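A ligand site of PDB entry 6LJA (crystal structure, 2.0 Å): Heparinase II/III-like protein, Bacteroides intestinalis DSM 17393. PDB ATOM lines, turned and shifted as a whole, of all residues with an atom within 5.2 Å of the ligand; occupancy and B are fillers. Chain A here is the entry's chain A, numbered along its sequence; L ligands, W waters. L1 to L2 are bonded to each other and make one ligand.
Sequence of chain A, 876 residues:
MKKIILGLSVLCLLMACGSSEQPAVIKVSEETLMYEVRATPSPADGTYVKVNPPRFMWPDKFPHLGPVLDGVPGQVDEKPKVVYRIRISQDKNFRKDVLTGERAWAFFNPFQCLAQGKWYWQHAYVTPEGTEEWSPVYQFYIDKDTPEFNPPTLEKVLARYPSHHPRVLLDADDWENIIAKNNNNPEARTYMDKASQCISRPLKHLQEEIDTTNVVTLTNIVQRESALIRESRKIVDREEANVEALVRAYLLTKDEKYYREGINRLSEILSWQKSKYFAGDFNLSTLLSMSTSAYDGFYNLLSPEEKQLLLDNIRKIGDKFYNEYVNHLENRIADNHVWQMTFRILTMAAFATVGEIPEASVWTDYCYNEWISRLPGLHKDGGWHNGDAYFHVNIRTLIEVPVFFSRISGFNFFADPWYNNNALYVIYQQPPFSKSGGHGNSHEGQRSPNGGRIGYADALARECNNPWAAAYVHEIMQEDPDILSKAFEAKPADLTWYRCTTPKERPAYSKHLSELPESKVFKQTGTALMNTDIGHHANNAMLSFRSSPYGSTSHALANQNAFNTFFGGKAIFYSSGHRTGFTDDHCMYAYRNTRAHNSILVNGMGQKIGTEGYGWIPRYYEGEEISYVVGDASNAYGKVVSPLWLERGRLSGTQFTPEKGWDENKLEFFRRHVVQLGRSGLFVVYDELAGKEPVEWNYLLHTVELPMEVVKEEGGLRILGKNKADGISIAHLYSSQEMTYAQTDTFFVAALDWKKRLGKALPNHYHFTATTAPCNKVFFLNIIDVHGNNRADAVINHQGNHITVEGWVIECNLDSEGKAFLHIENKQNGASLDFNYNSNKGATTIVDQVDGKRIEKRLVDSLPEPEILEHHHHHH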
ATOM      1  N   PRO A  67       1.103  27.213  24.225  1.00  0.00           N
ATOM      2  CA  PRO A  67       1.938  28.033  23.321  1.00  0.00           C
ATOM      3  C   PRO A  67       1.110  28.729  22.236  1.00  0.00           C
ATOM      4  O   PRO A  67       0.247  28.099  21.631  1.00  0.00           O
ATOM      5  CB  PRO A  67       2.865  27.005  22.677  1.00  0.00           C
ATOM      6  CG  PRO A  67       3.003  25.917  23.718  1.00  0.00           C
ATOM      7  CD  PRO A  67       1.655  25.859  24.408  1.00  0.00           C
ATOM      8  N   VAL A  68       1.375  30.007  21.985  1.00  0.00           N
ATOM      9  CA  VAL A  68       0.570  30.740  21.001  1.00  0.00           C
ATOM     10  C   VAL A  68       1.105  30.642  19.567  1.00  0.00           C
ATOM     11  O   VAL A  68       0.358  30.918  18.619  1.00  0.00           O
ATOM     12  CB  VAL A  68       0.373  32.215  21.413  1.00  0.00           C
ATOM     13  CG1 VAL A  68      -0.224  32.301  22.808  1.00  0.00           C
ATOM     14  CG2 VAL A  68       1.690  32.968  21.365  1.00  0.00           C
ATOM     15  N   LEU A  69       2.368  30.262  19.420  1.00  0.00           N
ATOM     16  CA  LEU A  69       2.964  30.062  18.088  1.00  0.00           C
ATOM     17  C   LEU A  69       3.920  28.867  18.102  1.00  0.00           C
ATOM     18  O   LEU A  69       4.432  28.497  19.165  1.00  0.00           O
ATOM     19  CB  LEU A  69       3.699  31.322  17.600  1.00  0.00           C
ATOM     20  CG  LEU A  69       2.859  32.576  17.292  1.00  0.00           C
ATOM     21  CD1 LEU A  69       3.740  33.821  17.168  1.00  0.00           C
ATOM     22  CD2 LEU A  69       2.039  32.379  16.021  1.00  0.00           C
ATOM     23  N   ASP A  70       4.156  28.263  16.942  1.00  0.00           N
ATOM     24  CA  ASP A  70       5.044  27.101  16.830  1.00  0.00           C
ATOM     25  C   ASP A  70       6.499  27.495  17.164  1.00  0.00           C
ATOM     26  O   ASP A  70       7.136  26.882  18.019  1.00  0.00           O
ATOM     27  CB  ASP A  70       4.936  26.516  15.415  1.00  0.00           C
ATOM     28  CG  ASP A  70       5.845  25.302  15.176  1.00  0.00           C
ATOM     29  OD1 ASP A  70       6.258  24.621  16.152  1.00  0.00           O
ATOM     30  OD2 ASP A  70       6.133  25.018  13.994  1.00  0.00           O
ATOM     31  N   GLY A  71       7.009  28.535  16.503  1.00  0.00           N
ATOM     32  CA  GLY A  71       8.373  28.952  16.755  1.00  0.00           C
ATOM     33  C   GLY A  71       8.614  29.680  18.072  1.00  0.00           C
ATOM     34  O   GLY A  71       9.730  29.695  18.591  1.00  0.00           O
ATOM     35  N   VAL A  72       7.574  30.324  18.593  1.00  0.00           N
ATOM     36  CA  VAL A  72       7.724  31.229  19.727  1.00  0.00           C
ATOM     37  C   VAL A  72       6.532  31.068  20.669  1.00  0.00           C
ATOM     38  O   VAL A  72       5.467  31.646  20.438  1.00  0.00           O
ATOM     39  CB  VAL A  72       7.813  32.702  19.245  1.00  0.00           C
ATOM     40  CG1 VAL A  72       7.948  33.647  20.422  1.00  0.00           C
ATOM     41  CG2 VAL A  72       8.987  32.896  18.281  1.00  0.00           C
ATOM     42  N   VAL A 222       9.779  36.314  15.639  1.00  0.00           N
ATOM     43  CA  VAL A 222       8.706  35.505  15.052  1.00  0.00           C
ATOM     44  C   VAL A 222       9.019  35.163  13.594  1.00  0.00           C
ATOM     45  O   VAL A 222       8.915  34.004  13.175  1.00  0.00           O
ATOM     46  CB  VAL A 222       7.323  36.168  15.176  1.00  0.00           C
ATOM     47  CG1 VAL A 222       6.267  35.344  14.455  1.00  0.00           C
ATOM     48  CG2 VAL A 222       6.935  36.343  16.649  1.00  0.00           C
ATOM     49  N   SER A 226      10.242  31.494  12.369  1.00  0.00           N
ATOM     50  CA  SER A 226       9.364  30.964  11.313  1.00  0.00           C
ATOM     51  C   SER A 226      10.130  30.550  10.058  1.00  0.00           C
ATOM     52  O   SER A 226       9.810  29.545   9.432  1.00  0.00           O
ATOM     53  CB  SER A 226       8.283  31.992  10.957  1.00  0.00           C
ATOM     54  OG  SER A 226       7.453  31.498   9.928  1.00  0.00           O
ATOM     55  N   ILE A 229      12.095  27.366  10.781  1.00  0.00           N
ATOM     56  CA  ILE A 229      11.148  26.249  10.637  1.00  0.00           C
ATOM     57  C   ILE A 229      11.018  25.842   9.177  1.00  0.00           C
ATOM     58  O   ILE A 229      11.184  24.663   8.818  1.00  0.00           O
ATOM     59  CB  ILE A 229       9.716  26.601  11.102  1.00  0.00           C
ATOM     60  CG1 ILE A 229       9.698  27.198  12.503  1.00  0.00           C
ATOM     61  CG2 ILE A 229       8.813  25.369  11.066  1.00  0.00           C
ATOM     62  CD1 ILE A 229      10.253  26.332  13.504  1.00  0.00           C
ATOM     63  N   ARG A 233      12.410  22.354   7.606  1.00  0.00           N
ATOM     64  CA  ARG A 233      11.365  21.461   7.121  1.00  0.00           C
ATOM     65  C   ARG A 233      11.583  21.099   5.647  1.00  0.00           C
ATOM     66  O   ARG A 233      11.256  19.992   5.240  1.00  0.00           O
ATOM     67  CB  ARG A 233       9.956  22.076   7.309  1.00  0.00           C
ATOM     68  CG  ARG A 233       9.443  22.105   8.772  1.00  0.00           C
ATOM     69  CD  ARG A 233       7.945  22.330   8.808  1.00  0.00           C
ATOM     70  NE  ARG A 233       7.287  21.323   7.977  1.00  0.00           N
ATOM     71  CZ  ARG A 233       6.110  21.479   7.377  1.00  0.00           C
ATOM     72  NH1 ARG A 233       5.419  22.606   7.536  1.00  0.00           N
ATOM     73  NH2 ARG A 233       5.634  20.507   6.622  1.00  0.00           N
ATOM     74  N   PHE A 282       6.470  20.117  13.555  1.00  0.00           N
ATOM     75  CA  PHE A 282       6.305  19.182  12.442  1.00  0.00           C
ATOM     76  C   PHE A 282       7.574  18.335  12.249  1.00  0.00           C
ATOM     77  O   PHE A 282       7.475  17.115  12.057  1.00  0.00           O
ATOM     78  CB  PHE A 282       5.917  19.875  11.140  1.00  0.00           C
ATOM     79  CG  PHE A 282       4.428  20.195  11.022  1.00  0.00           C
ATOM     80  CD1 PHE A 282       3.467  19.329  11.528  1.00  0.00           C
ATOM     81  CD2 PHE A 282       4.008  21.373  10.402  1.00  0.00           C
ATOM     82  CE1 PHE A 282       2.105  19.617  11.415  1.00  0.00           C
ATOM     83  CE2 PHE A 282       2.644  21.668  10.296  1.00  0.00           C
ATOM     84  CZ  PHE A 282       1.697  20.787  10.793  1.00  0.00           C
ATOM     85  N   ARG A 332      -9.148  22.824  22.831  1.00  0.00           N
ATOM     86  CA  ARG A 332      -8.849  23.916  21.904  1.00  0.00           C
ATOM     87  C   ARG A 332      -9.935  23.939  20.826  1.00  0.00           C
ATOM     88  O   ARG A 332     -10.486  22.883  20.502  1.00  0.00           O
ATOM     89  CB  ARG A 332      -7.487  23.698  21.248  1.00  0.00           C
ATOM     90  CG  ARG A 332      -6.310  24.000  22.158  1.00  0.00           C
ATOM     91  CD  ARG A 332      -6.080  25.506  22.317  1.00  0.00           C
ATOM     92  NE  ARG A 332      -5.472  26.103  21.127  1.00  0.00           N
ATOM     93  CZ  ARG A 332      -6.008  27.099  20.421  1.00  0.00           C
ATOM     94  NH1 ARG A 332      -7.165  27.657  20.767  1.00  0.00           N
ATOM     95  NH2 ARG A 332      -5.357  27.558  19.360  1.00  0.00           N
ATOM     96  N   ALA A 334      -9.608  24.316  17.752  1.00  0.00           N
ATOM     97  CA  ALA A 334      -8.952  23.381  16.838  1.00  0.00           C
ATOM     98  C   ALA A 334      -7.464  23.676  17.008  1.00  0.00           C
ATOM     99  O   ALA A 334      -7.084  24.846  17.138  1.00  0.00           O
ATOM    100  CB  ALA A 334      -9.392  23.615  15.406  1.00  0.00           C
ATOM    101  N   ASP A 335      -6.628  22.646  17.038  1.00  0.00           N
ATOM    102  CA  ASP A 335      -5.187  22.835  17.232  1.00  0.00           C
ATOM    103  C   ASP A 335      -4.544  22.401  15.923  1.00  0.00           C
ATOM    104  O   ASP A 335      -4.386  21.211  15.670  1.00  0.00           O
ATOM    105  CB  ASP A 335      -4.724  21.930  18.391  1.00  0.00           C
ATOM    106  CG  ASP A 335      -3.351  22.307  18.936  1.00  0.00           C
ATOM    107  OD1 ASP A 335      -2.544  22.955  18.251  1.00  0.00           O
ATOM    108  OD2 ASP A 335      -3.063  21.909  20.084  1.00  0.00           O
ATOM    109  N   ASN A 336      -4.196  23.381  15.074  1.00  0.00           N
ATOM    110  CA  ASN A 336      -3.885  23.133  13.669  1.00  0.00           C
ATOM    111  C   ASN A 336      -2.878  22.042  13.352  1.00  0.00           C
ATOM    112  O   ASN A 336      -3.160  21.121  12.578  1.00  0.00           O
ATOM    113  CB  ASN A 336      -3.462  24.438  12.984  1.00  0.00           C
ATOM    114  CG  ASN A 336      -4.578  25.451  12.926  1.00  0.00           C
ATOM    115  OD1 ASN A 336      -5.743  25.106  13.117  1.00  0.00           O
ATOM    116  ND2 ASN A 336      -4.232  26.708  12.665  1.00  0.00           N
ATOM    117  N   HIS A 337      -1.676  22.130  13.920  1.00  0.00           N
ATOM    118  CA  HIS A 337      -0.627  21.183  13.555  1.00  0.00           C
ATOM    119  C   HIS A 337      -1.008  19.799  14.018  1.00  0.00           C
ATOM    120  O   HIS A 337      -0.621  18.794  13.410  1.00  0.00           O
ATOM    121  CB  HIS A 337       0.721  21.591  14.161  1.00  0.00           C
ATOM    122  CG  HIS A 337       1.325  22.793  13.511  1.00  0.00           C
ATOM    123  ND1 HIS A 337       2.640  23.160  13.735  1.00  0.00           N
ATOM    124  CD2 HIS A 337       0.814  23.692  12.636  1.00  0.00           C
ATOM    125  CE1 HIS A 337       2.901  24.245  13.025  1.00  0.00           C
ATOM    126  NE2 HIS A 337       1.814  24.587  12.356  1.00  0.00           N
ATOM    127  N   GLN A 340      -3.910  18.494  11.688  1.00  0.00           N
ATOM    128  CA  GLN A 340      -3.328  18.230  10.368  1.00  0.00           C
ATOM    129  C   GLN A 340      -2.512  16.934  10.298  1.00  0.00           C
ATOM    130  O   GLN A 340      -2.790  16.060   9.482  1.00  0.00           O
ATOM    131  CB  GLN A 340      -2.469  19.425   9.930  1.00  0.00           C
ATOM    132  CG  GLN A 340      -3.321  20.634   9.518  1.00  0.00           C
ATOM    133  CD  GLN A 340      -2.549  21.926   9.564  1.00  0.00           C
ATOM    134  OE1 GLN A 340      -1.335  21.932   9.760  1.00  0.00           O
ATOM    135  NE2 GLN A 340      -3.259  23.041   9.389  1.00  0.00           N
ATOM    136  N   TYR A 390      -5.886  24.929   3.578  1.00  0.00           N
ATOM    137  CA  TYR A 390      -5.526  24.085   4.714  1.00  0.00           C
ATOM    138  C   TYR A 390      -6.332  22.804   4.856  1.00  0.00           C
ATOM    139  O   TYR A 390      -5.882  21.871   5.501  1.00  0.00           O
ATOM    140  CB  TYR A 390      -5.457  24.870   6.029  1.00  0.00           C
ATOM    141  CG  TYR A 390      -4.104  25.518   6.134  1.00  0.00           C
ATOM    142  CD1 TYR A 390      -2.983  24.759   6.481  1.00  0.00           C
ATOM    143  CD2 TYR A 390      -3.919  26.845   5.807  1.00  0.00           C
ATOM    144  CE1 TYR A 390      -1.739  25.328   6.535  1.00  0.00           C
ATOM    145  CE2 TYR A 390      -2.667  27.429   5.850  1.00  0.00           C
ATOM    146  CZ  TYR A 390      -1.581  26.663   6.219  1.00  0.00           C
ATOM    147  OH  TYR A 390      -0.345  27.233   6.269  1.00  0.00           O
ATOM    148  N   VAL A 393      -4.195  19.778   4.017  1.00  0.00           N
ATOM    149  CA  VAL A 393      -3.138  19.403   4.946  1.00  0.00           C
ATOM    150  C   VAL A 393      -3.690  18.411   5.984  1.00  0.00           C
ATOM    151  O   VAL A 393      -2.937  17.804   6.762  1.00  0.00           O
ATOM    152  CB  VAL A 393      -2.522  20.667   5.608  1.00  0.00           C
ATOM    153  CG1 VAL A 393      -1.287  20.315   6.452  1.00  0.00           C
ATOM    154  CG2 VAL A 393      -2.122  21.683   4.520  1.00  0.00           C
ATOM    155  N   SER A 554      -7.229  31.640  13.897  1.00  0.00           N
ATOM    156  CA  SER A 554      -6.526  30.572  13.195  1.00  0.00           C
ATOM    157  C   SER A 554      -6.164  30.926  11.732  1.00  0.00           C
ATOM    158  O   SER A 554      -5.523  31.945  11.489  1.00  0.00           O
ATOM    159  CB  SER A 554      -7.340  29.283  13.286  1.00  0.00           C
ATOM    160  OG  SER A 554      -6.557  28.130  13.044  1.00  0.00           O
ATOM    161  N   HIS A 555      -6.555  30.091  10.768  1.00  0.00           N
ATOM    162  CA  HIS A 555      -6.290  30.411   9.358  1.00  0.00           C
ATOM    163  C   HIS A 555      -7.438  31.125   8.662  1.00  0.00           C
ATOM    164  O   HIS A 555      -7.365  31.379   7.468  1.00  0.00           O
ATOM    165  CB  HIS A 555      -5.970  29.149   8.540  1.00  0.00           C
ATOM    166  CG  HIS A 555      -4.625  28.550   8.836  1.00  0.00           C
ATOM    167  ND1 HIS A 555      -3.453  29.254   8.682  1.00  0.00           N
ATOM    168  CD2 HIS A 555      -4.283  27.315   9.255  1.00  0.00           C
ATOM    169  CE1 HIS A 555      -2.430  28.483   9.020  1.00  0.00           C
ATOM    170  NE2 HIS A 555      -2.907  27.297   9.364  1.00  0.00           N
ATOM    171  N   ARG A 579      -0.876  35.719   1.017  1.00  0.00           N
ATOM    172  CA  ARG A 579      -0.475  35.033   2.247  1.00  0.00           C
ATOM    173  C   ARG A 579       1.062  35.006   2.323  1.00  0.00           C
ATOM    174  O   ARG A 579       1.708  34.147   1.703  1.00  0.00           O
ATOM    175  CB  ARG A 579      -1.030  33.610   2.274  1.00  0.00           C
ATOM    176  CG  ARG A 579      -1.017  32.936   3.662  1.00  0.00           C
ATOM    177  CD  ARG A 579       0.282  32.215   3.926  1.00  0.00           C
ATOM    178  NE  ARG A 579       0.327  31.555   5.228  1.00  0.00           N
ATOM    179  CZ  ARG A 579       0.011  30.278   5.447  1.00  0.00           C
ATOM    180  NH1 ARG A 579      -0.397  29.500   4.439  1.00  0.00           N
ATOM    181  NH2 ARG A 579       0.091  29.774   6.674  1.00  0.00           N
ATOM    182  N   GLY A 581       2.674  35.110   5.447  1.00  0.00           N
ATOM    183  CA  GLY A 581       3.026  34.583   6.752  1.00  0.00           C
ATOM    184  C   GLY A 581       1.794  34.205   7.556  1.00  0.00           C
ATOM    185  O   GLY A 581       0.754  33.870   6.980  1.00  0.00           O
ATOM    186  N   PHE A 582       1.908  34.236   8.878  1.00  0.00           N
ATOM    187  CA  PHE A 582       0.784  33.878   9.744  1.00  0.00           C
ATOM    188  C   PHE A 582       0.365  35.057  10.602  1.00  0.00           C
ATOM    189  O   PHE A 582      -0.830  35.233  10.878  1.00  0.00           O
ATOM    190  CB  PHE A 582       1.147  32.675  10.634  1.00  0.00           C
ATOM    191  CG  PHE A 582      -0.025  32.128  11.431  1.00  0.00           C
ATOM    192  CD1 PHE A 582      -1.072  31.464  10.805  1.00  0.00           C
ATOM    193  CD2 PHE A 582      -0.041  32.242  12.814  1.00  0.00           C
ATOM    194  CE1 PHE A 582      -2.134  30.923  11.538  1.00  0.00           C
ATOM    195  CE2 PHE A 582      -1.099  31.713  13.566  1.00  0.00           C
ATOM    196  CZ  PHE A 582      -2.154  31.059  12.912  1.00  0.00           C
ATOM    197  N   ARG A 648      -0.122  37.152  20.268  1.00  0.00           N
ATOM    198  CA  ARG A 648       0.547  37.036  18.970  1.00  0.00           C
ATOM    199  C   ARG A 648       0.964  38.416  18.453  1.00  0.00           C
ATOM    200  O   ARG A 648       2.059  38.578  17.898  1.00  0.00           O
ATOM    201  CB  ARG A 648      -0.356  36.310  17.959  1.00  0.00           C
ATOM    202  CG  ARG A 648      -0.416  34.826  18.194  1.00  0.00           C
ATOM    203  CD  ARG A 648      -1.405  34.132  17.278  1.00  0.00           C
ATOM    204  NE  ARG A 648      -1.348  32.678  17.486  1.00  0.00           N
ATOM    205  CZ  ARG A 648      -2.288  31.826  17.072  1.00  0.00           C
ATOM    206  NH1 ARG A 648      -3.351  32.270  16.430  1.00  0.00           N
ATOM    207  NH2 ARG A 648      -2.146  30.526  17.309  1.00  0.00           N
HETATM  208  C1  LIG L   1       0.288  27.874  15.656  1.00  0.00           C
HETATM  209  C2  LIG L   1      -0.869  27.649  14.682  1.00  0.00           C
HETATM  210  C3  LIG L   1      -0.324  27.184  13.337  1.00  0.00           C
HETATM  211  C4  LIG L   1       0.774  28.105  12.815  1.00  0.00           C
HETATM  212  C5  LIG L   1       1.806  28.399  13.906  1.00  0.00           C
HETATM  213  C6  LIG L   1       2.758  29.458  13.401  1.00  0.00           C
HETATM  214  N1  LIG L   1      -1.790  26.607  15.196  1.00  0.00           N
HETATM  215  O1  LIG L   1       0.998  26.640  15.869  1.00  0.00           O
HETATM  216  O2  LIG L   1      -1.386  27.105  12.390  1.00  0.00           O
HETATM  217  O3  LIG L   1       1.466  27.464  11.744  1.00  0.00           O
HETATM  218  O4  LIG L   1       1.185  28.843  15.101  1.00  0.00           O
HETATM  219  O5  LIG L   1       3.916  29.543  14.222  1.00  0.00           O
HETATM  220  S1  LIG L   1      -2.981  27.228  16.092  1.00  0.00           S
HETATM  221  O6  LIG L   1      -2.487  27.599  17.436  1.00  0.00           O
HETATM  222  O7  LIG L   1      -3.593  28.417  15.433  1.00  0.00           O
HETATM  223  O8  LIG L   1      -4.014  26.174  16.210  1.00  0.00           O
HETATM  224  S2  LIG L   1       5.128  30.369  13.717  1.00  0.00           S
HETATM  225  O9  LIG L   1       5.680  29.740  12.499  1.00  0.00           O
HETATM  226  O10 LIG L   1       4.681  31.742  13.414  1.00  0.00           O
HETATM  227  O11 LIG L   1       6.159  30.417  14.766  1.00  0.00           O
HETATM  228  S1  LG2 L   2       3.302  30.139   8.180  1.00  0.00           S
HETATM  229  C1  LG2 L   2       1.264  28.096  10.481  1.00  0.00           C
HETATM  230  C2  LG2 L   2       2.583  28.164   9.714  1.00  0.00           C
HETATM  231  O1  LG2 L   2       2.337  28.986   8.570  1.00  0.00           O
HETATM  232  C3  LG2 L   2       3.126  26.781   9.329  1.00  0.00           C
HETATM  233  O2  LG2 L   2       3.669  26.162  10.492  1.00  0.00           O
HETATM  234  C4  LG2 L   2       2.006  25.914   8.778  1.00  0.00           C
HETATM  235  C5  LG2 L   2       0.782  26.066   9.292  1.00  0.00           C
HETATM  236  O3  LG2 L   2       0.316  27.392   9.687  1.00  0.00           O
HETATM  237  C6  LG2 L   2      -0.113  24.923   9.471  1.00  0.00           C
HETATM  238  O4  LG2 L   2       4.285  29.630   7.190  1.00  0.00           O
HETATM  239  O5  LG2 L   2       2.550  31.250   7.558  1.00  0.00           O
HETATM  240  O6  LG2 L   2       4.033  30.628   9.389  1.00  0.00           O
HETATM  241  O7  LG2 L   2       0.240  23.807   8.996  1.00  0.00           O
HETATM  242  O8  LG2 L   2      -1.177  25.093  10.097  1.00  0.00           O
HETATM  243  O   HOH W   1       5.528  24.372   9.960  1.00  0.00           O
HETATM  244  O   HOH W   2      -6.847  26.972  15.669  1.00  0.00           O
HETATM  245  O   HOH W   3       2.092  25.961  18.303  1.00  0.00           O
HETATM  246  O   HOH W   4      -0.991  23.960  16.071  1.00  0.00           O
HETATM  247  O   HOH W   5      -5.300  30.305  16.071  1.00  0.00           O
HETATM  248  O   HOH W   6       5.675  27.214  12.109  1.00  0.00           O
HETATM  249  O   HOH W   7      -0.082  27.535  19.130  1.00  0.00           O
HETATM  250  O   HOH W   8      -2.957  25.402  20.040  1.00  0.00           O
HETATM  251  O   HOH W   9       6.616  28.490   5.160  1.00  0.00           O
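O6 of LIG L1 is in salt-bridge range of NH2 of Arg 332 (3.5 Å). OH of Tyr 390 sits close to O3 of LG2 L2 (3.5 Å). OE1 of Gln 340 sits close to O7 of LG2 L2 (2.6 Å). O6 of LIG L1 lies within salt-bridge range of NH2 of Arg 648. N of Gly 71 lies within hydrogen-bond range of O11 of LIG L1. The backbone NH (N) of Asp 70 lies within hydrogen-bond range of an oxygen (O5) of LIG L1, at 3.0 Å. The side-chain amide nitrogen (ND2) of Asn 336 lies within hydrogen-bond range of an oxygen (O2) of LIG L1 (2.9 Å). A ring nitrogen (NE2) of His 555 lies within hydrogen-bond range of an oxygen (O8) of LG2 L2 (2.9 Å). The guanidinium group of Arg 579 lies within salt-bridge range of an oxygen (O5) of LG2 L2, at 3.0 Å. N of Asn 336 lies within hydrogen-bond range of O8 of LIG L1 (3.0 Å). A ring nitrogen (NE2) of His 337 sits at hydrogen-bond distance from an oxygen (O3) of LIG L1 (3.0 Å). N of Phe 582 lies within hydrogen-bond range of O5 of LG2 L2 (3.3 Å).
NH2 of Arg 579 lies within hydrogen-bond range of OH of Tyr 390 (2.6 Å). The side-chain amide nitrogen (ND2) of Asn 336 is in hydrogen-bond range of the side-chain hydroxyl (OG) of Ser 554 (2.8 Å). The guanidinium group of Arg 579 lies within hydrogen-bond range of the backbone carbonyl oxygen of Gly 581, at 2.9 Å. The side-chain amide oxygen (OE1) of Gln 340 sits close to the backbone carbonyl oxygen (O) of Asn 336 (3.5 Å). The backbone carbonyl oxygen (O) of Val 68 is in hydrogen-bond range of the guanidinium group (NE) of Arg 648, at 2.7 Å.
An oxygen (O8) of LIG L1 sits close to the backbone carbonyl oxygen (O) of Ala 334 (3.5 Å). The backbone carbonyl oxygen of Gly 581 lies close to an oxygen (O5) of LG2 L2 (3.2 Å). Leu 69 touches the ligand. OG of Ser 226 touches O6 of LG2 L2, 3.6 Å away. Phe 282 touches the ligand. CA of Asp 335 touches O8 of LIG L1 (3.7 Å). Ser 554 touches the ligand. Hydrophobic or aromatic side chains that line the ligand: Leu 69, Phe 282, His 337, Tyr 390, His 555 and Phe 582. Of the 25 residues printed, 18 come within 4 Å of the ligand.
Water W6 lies within hydrogen-bond range of O9 of LIG L1 (2.6 Å) and OD2 of Asp 70 (2.9 Å). Water W5 lies within hydrogen-bond range of O7 of LIG L1 (2.6 Å), NH1 of Arg 648 (2.8 Å) and N of Ser 554 (3.2 Å). Water W3 bridges an oxygen (O1) of LIG L1 (2.8 Å) and the backbone NH (N) of Asp 70 (3.4 Å). Water W7 lies within hydrogen-bond range of O of Pro 67 (2.6 Å), O6 of LIG L1 (2.9 Å) and O of Val 68 (3.4 Å). Water W2 lies within hydrogen-bond range of the backbone carbonyl oxygen of Ala 334 (2.6 Å), the side-chain hydroxyl of Ser 554 (2.9 Å), an oxygen (O8) of LIG L1 (3.0 Å) and the side-chain amide oxygen of Asn 336 (3.3 Å). Water W8 lies within hydrogen-bond range of the guanidinium group of Arg 332, the side-chain carboxylate of Asp 335 and an oxygen (O6) of LIG L1.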
